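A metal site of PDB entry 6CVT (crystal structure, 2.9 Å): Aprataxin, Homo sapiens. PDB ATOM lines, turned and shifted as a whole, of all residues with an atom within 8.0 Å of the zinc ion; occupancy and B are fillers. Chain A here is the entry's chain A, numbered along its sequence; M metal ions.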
ATOM      1  N   TRP A 119      11.073 -16.307 -22.533  1.00  0.00           N
ATOM      2  CA  TRP A 119       9.655 -16.273 -22.863  1.00  0.00           C
ATOM      3  C   TRP A 119       9.146 -17.644 -23.249  1.00  0.00           C
ATOM      4  O   TRP A 119       8.117 -18.114 -22.747  1.00  0.00           O
ATOM      5  CB  TRP A 119       9.383 -15.263 -23.982  1.00  0.00           C
ATOM      6  CG  TRP A 119       7.933 -15.229 -24.272  1.00  0.00           C
ATOM      7  CD1 TRP A 119       7.288 -15.818 -25.309  1.00  0.00           C
ATOM      8  CD2 TRP A 119       6.922 -14.651 -23.441  1.00  0.00           C
ATOM      9  NE1 TRP A 119       5.929 -15.607 -25.204  1.00  0.00           N
ATOM     10  CE2 TRP A 119       5.679 -14.901 -24.058  1.00  0.00           C
ATOM     11  CE3 TRP A 119       6.941 -13.930 -22.243  1.00  0.00           C
ATOM     12  CZ2 TRP A 119       4.490 -14.447 -23.524  1.00  0.00           C
ATOM     13  CZ3 TRP A 119       5.755 -13.483 -21.704  1.00  0.00           C
ATOM     14  CH2 TRP A 119       4.542 -13.738 -22.349  1.00  0.00           C
ATOM     15  N   ARG A 158       4.938 -15.348 -29.187  1.00  0.00           N
ATOM     16  CA  ARG A 158       3.486 -15.289 -29.240  1.00  0.00           C
ATOM     17  C   ARG A 158       2.939 -14.993 -27.859  1.00  0.00           C
ATOM     18  O   ARG A 158       3.295 -15.674 -26.898  1.00  0.00           O
ATOM     19  CB  ARG A 158       2.884 -16.586 -29.773  1.00  0.00           C
ATOM     20  CG  ARG A 158       1.380 -16.553 -29.843  1.00  0.00           C
ATOM     21  CD  ARG A 158       0.830 -17.875 -30.354  1.00  0.00           C
ATOM     22  NE  ARG A 158       1.262 -18.175 -31.716  1.00  0.00           N
ATOM     23  CZ  ARG A 158       0.599 -17.815 -32.805  1.00  0.00           C
ATOM     24  NH1 ARG A 158      -0.541 -17.134 -32.691  1.00  0.00           N
ATOM     25  NH2 ARG A 158       1.054 -18.126 -34.015  1.00  0.00           N
ATOM     26  N   CYS A 159       2.076 -13.987 -27.771  1.00  0.00           N
ATOM     27  CA  CYS A 159       1.493 -13.596 -26.490  1.00  0.00           C
ATOM     28  C   CYS A 159       0.636 -14.721 -25.938  1.00  0.00           C
ATOM     29  O   CYS A 159      -0.102 -15.375 -26.671  1.00  0.00           O
ATOM     30  CB  CYS A 159       0.660 -12.328 -26.653  1.00  0.00           C
ATOM     31  SG  CYS A 159      -0.300 -11.921 -25.179  1.00  0.00           S
ATOM     32  N   HIS A 160       0.716 -14.925 -24.613  1.00  0.00           N
ATOM     33  CA  HIS A 160      -0.034 -16.005 -23.984  1.00  0.00           C
ATOM     34  C   HIS A 160      -1.484 -15.661 -23.709  1.00  0.00           C
ATOM     35  O   HIS A 160      -2.280 -16.577 -23.446  1.00  0.00           O
ATOM     36  CB  HIS A 160       0.669 -16.421 -22.690  1.00  0.00           C
ATOM     37  CG  HIS A 160       0.718 -15.343 -21.648  1.00  0.00           C
ATOM     38  ND1 HIS A 160       1.358 -14.142 -21.856  1.00  0.00           N
ATOM     39  CD2 HIS A 160       0.226 -15.295 -20.385  1.00  0.00           C
ATOM     40  CE1 HIS A 160       1.253 -13.395 -20.773  1.00  0.00           C
ATOM     41  NE2 HIS A 160       0.573 -14.068 -19.861  1.00  0.00           N
ATOM     42  N   GLU A 161      -1.858 -14.388 -23.766  1.00  0.00           N
ATOM     43  CA  GLU A 161      -3.231 -13.974 -23.523  1.00  0.00           C
ATOM     44  C   GLU A 161      -3.969 -13.811 -24.845  1.00  0.00           C
ATOM     45  O   GLU A 161      -4.828 -14.623 -25.197  1.00  0.00           O
ATOM     46  CB  GLU A 161      -3.270 -12.674 -22.704  1.00  0.00           C
ATOM     47  CG  GLU A 161      -2.468 -12.681 -21.416  1.00  0.00           C
ATOM     48  CD  GLU A 161      -3.241 -13.192 -20.202  1.00  0.00           C
ATOM     49  OE1 GLU A 161      -4.031 -14.162 -20.343  1.00  0.00           O
ATOM     50  OE2 GLU A 161      -3.040 -12.630 -19.110  1.00  0.00           O
ATOM     51  N   CYS A 162      -3.655 -12.735 -25.576  1.00  0.00           N
ATOM     52  CA  CYS A 162      -4.354 -12.414 -26.820  1.00  0.00           C
ATOM     53  C   CYS A 162      -4.043 -13.404 -27.937  1.00  0.00           C
ATOM     54  O   CYS A 162      -4.873 -13.589 -28.827  1.00  0.00           O
ATOM     55  CB  CYS A 162      -4.011 -11.001 -27.261  1.00  0.00           C
ATOM     56  SG  CYS A 162      -2.355 -10.819 -27.971  1.00  0.00           S
ATOM     57  N   GLN A 163      -2.859 -14.014 -27.914  1.00  0.00           N
ATOM     58  CA  GLN A 163      -2.324 -14.999 -28.890  1.00  0.00           C
ATOM     59  C   GLN A 163      -1.753 -14.372 -30.152  1.00  0.00           C
ATOM     60  O   GLN A 163      -1.529 -15.097 -31.142  1.00  0.00           O
ATOM     61  CB  GLN A 163      -3.363 -16.056 -29.302  1.00  0.00           C
ATOM     62  CG  GLN A 163      -3.816 -16.940 -28.159  1.00  0.00           C
ATOM     63  CD  GLN A 163      -2.722 -17.855 -27.667  1.00  0.00           C
ATOM     64  OE1 GLN A 163      -1.898 -18.334 -28.452  1.00  0.00           O
ATOM     65  NE2 GLN A 163      -2.685 -18.096 -26.361  1.00  0.00           N
ATOM     66  N   GLN A 164      -1.499 -13.070 -30.153  1.00  0.00           N
ATOM     67  CA  GLN A 164      -0.917 -12.397 -31.306  1.00  0.00           C
ATOM     68  C   GLN A 164       0.586 -12.646 -31.381  1.00  0.00           C
ATOM     69  O   GLN A 164       1.280 -12.648 -30.357  1.00  0.00           O
ATOM     70  CB  GLN A 164      -1.198 -10.905 -31.242  1.00  0.00           C
ATOM     71  CG  GLN A 164      -0.666 -10.064 -32.388  1.00  0.00           C
ATOM     72  CD  GLN A 164      -0.587  -8.600 -31.993  1.00  0.00           C
ATOM     73  OE1 GLN A 164      -1.444  -8.100 -31.266  1.00  0.00           O
ATOM     74  NE2 GLN A 164       0.433  -7.896 -32.481  1.00  0.00           N
ATOM     75  N   LEU A 165       1.101 -12.831 -32.591  1.00  0.00           N
ATOM     76  CA  LEU A 165       2.542 -12.953 -32.797  1.00  0.00           C
ATOM     77  C   LEU A 165       3.199 -11.592 -32.634  1.00  0.00           C
ATOM     78  O   LEU A 165       2.660 -10.577 -33.072  1.00  0.00           O
ATOM     79  CB  LEU A 165       2.826 -13.524 -34.185  1.00  0.00           C
ATOM     80  CG  LEU A 165       2.415 -14.982 -34.376  1.00  0.00           C
ATOM     81  CD1 LEU A 165       2.460 -15.379 -35.835  1.00  0.00           C
ATOM     82  CD2 LEU A 165       3.392 -15.818 -33.584  1.00  0.00           C
ATOM     83  N   LEU A 166       4.373 -11.574 -32.011  1.00  0.00           N
ATOM     84  CA  LEU A 166       5.107 -10.344 -31.771  1.00  0.00           C
ATOM     85  C   LEU A 166       6.552 -10.462 -32.246  1.00  0.00           C
ATOM     86  O   LEU A 166       7.111 -11.565 -32.307  1.00  0.00           O
ATOM     87  CB  LEU A 166       5.055  -9.991 -30.275  1.00  0.00           C
ATOM     88  CG  LEU A 166       3.688  -9.419 -29.876  1.00  0.00           C
ATOM     89  CD1 LEU A 166       3.573  -9.281 -28.390  1.00  0.00           C
ATOM     90  CD2 LEU A 166       3.423  -8.093 -30.557  1.00  0.00           C
ATOM     91  N   LEU A 172       7.061  -7.084 -27.255  1.00  0.00           N
ATOM     92  CA  LEU A 172       6.293  -8.026 -26.444  1.00  0.00           C
ATOM     93  C   LEU A 172       5.961  -7.434 -25.085  1.00  0.00           C
ATOM     94  O   LEU A 172       4.821  -7.536 -24.628  1.00  0.00           O
ATOM     95  CB  LEU A 172       7.065  -9.317 -26.252  1.00  0.00           C
ATOM     96  CG  LEU A 172       6.449 -10.294 -25.250  1.00  0.00           C
ATOM     97  CD1 LEU A 172       5.076 -10.789 -25.670  1.00  0.00           C
ATOM     98  CD2 LEU A 172       7.398 -11.463 -24.944  1.00  0.00           C
ATOM     99  N   HIS A 175       3.342  -4.836 -25.444  1.00  0.00           N
ATOM    100  CA  HIS A 175       2.060  -5.479 -25.692  1.00  0.00           C
ATOM    101  C   HIS A 175       1.472  -6.047 -24.412  1.00  0.00           C
ATOM    102  O   HIS A 175       0.263  -5.970 -24.173  1.00  0.00           O
ATOM    103  CB  HIS A 175       2.220  -6.562 -26.758  1.00  0.00           C
ATOM    104  CG  HIS A 175       1.085  -7.538 -26.830  1.00  0.00           C
ATOM    105  ND1 HIS A 175      -0.114  -7.237 -27.442  1.00  0.00           N
ATOM    106  CD2 HIS A 175       0.967  -8.804 -26.365  1.00  0.00           C
ATOM    107  CE1 HIS A 175      -0.923  -8.275 -27.352  1.00  0.00           C
ATOM    108  NE2 HIS A 175      -0.291  -9.248 -26.705  1.00  0.00           N
ATOM    109  N   LEU A 176       2.333  -6.605 -23.546  1.00  0.00           N
ATOM    110  CA  LEU A 176       1.845  -7.134 -22.282  1.00  0.00           C
ATOM    111  C   LEU A 176       1.315  -6.026 -21.397  1.00  0.00           C
ATOM    112  O   LEU A 176       0.283  -6.197 -20.745  1.00  0.00           O
ATOM    113  CB  LEU A 176       2.959  -7.914 -21.564  1.00  0.00           C
ATOM    114  CG  LEU A 176       3.477  -9.189 -22.229  1.00  0.00           C
ATOM    115  CD1 LEU A 176       4.468  -9.915 -21.336  1.00  0.00           C
ATOM    116  CD2 LEU A 176       2.331 -10.105 -22.577  1.00  0.00           C
ATOM    117  N   ARG A 177       1.998  -4.864 -21.378  1.00  0.00           N
ATOM    118  CA  ARG A 177       1.573  -3.733 -20.554  1.00  0.00           C
ATOM    119  C   ARG A 177       0.084  -3.497 -20.671  1.00  0.00           C
ATOM    120  O   ARG A 177      -0.603  -3.261 -19.672  1.00  0.00           O
ATOM    121  CB  ARG A 177       2.321  -2.450 -20.944  1.00  0.00           C
ATOM    122  CG  ARG A 177       3.855  -2.475 -20.829  1.00  0.00           C
ATOM    123  CD  ARG A 177       4.345  -2.305 -19.395  1.00  0.00           C
ATOM    124  NE  ARG A 177       5.801  -2.317 -19.316  1.00  0.00           N
ATOM    125  CZ  ARG A 177       6.537  -3.416 -19.130  1.00  0.00           C
ATOM    126  NH1 ARG A 177       5.951  -4.607 -19.002  1.00  0.00           N
ATOM    127  NH2 ARG A 177       7.868  -3.334 -19.074  1.00  0.00           N
ATOM    128  N   LYS A 178      -0.443  -3.592 -21.887  1.00  0.00           N
ATOM    129  CA  LYS A 178      -1.837  -3.256 -22.099  1.00  0.00           C
ATOM    130  C   LYS A 178      -2.795  -4.319 -21.593  1.00  0.00           C
ATOM    131  O   LYS A 178      -3.998  -4.055 -21.507  1.00  0.00           O
ATOM    132  CB  LYS A 178      -2.025  -2.950 -23.593  1.00  0.00           C
ATOM    133  CG  LYS A 178      -1.148  -1.747 -23.962  1.00  0.00           C
ATOM    134  CD  LYS A 178      -1.019  -1.502 -25.432  1.00  0.00           C
ATOM    135  CE  LYS A 178      -0.028  -0.358 -25.669  1.00  0.00           C
ATOM    136  NZ  LYS A 178       0.159  -0.064 -27.113  1.00  0.00           N
ATOM    137  N   HIS A 179      -2.314  -5.492 -21.220  1.00  0.00           N
ATOM    138  CA  HIS A 179      -3.185  -6.528 -20.684  1.00  0.00           C
ATOM    139  C   HIS A 179      -3.415  -6.395 -19.178  1.00  0.00           C
ATOM    140  O   HIS A 179      -3.900  -7.343 -18.555  1.00  0.00           O
ATOM    141  CB  HIS A 179      -2.615  -7.916 -20.973  1.00  0.00           C
ATOM    142  CG  HIS A 179      -3.028  -8.479 -22.300  1.00  0.00           C
ATOM    143  ND1 HIS A 179      -4.186  -9.208 -22.477  1.00  0.00           N
ATOM    144  CD2 HIS A 179      -2.405  -8.458 -23.490  1.00  0.00           C
ATOM    145  CE1 HIS A 179      -4.265  -9.578 -23.741  1.00  0.00           C
ATOM    146  NE2 HIS A 179      -3.179  -9.152 -24.379  1.00  0.00           N
HETATM  147 ZN    ZN M   1      -1.892 -10.237 -25.796  1.00  0.00          ZN
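Along chain A the residues within 4 Å of the zinc ion span positions 159 to 179.
The zinc ion is bound by a ring nitrogen (NE2) of His 175 (2.1 Å), a ring nitrogen (NE2) of His 179 (2.2 Å), the side-chain sulfur of Cys 162 (2.3 Å) and the side-chain sulfur of Cys 159 (2.4 Å).
The zinc ion has four donor atoms within binding distance.
SG of Cys 162 lies close to N of Gln 164, at 3.2 Å.
N of Cys 159 sits at hydrogen-bond distance from O of Gln 164, at 3.0 Å.
The side-chain sulfur (SG) of Cys 159 sits close to the backbone NH (N) of Glu 161 (3.2 Å).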
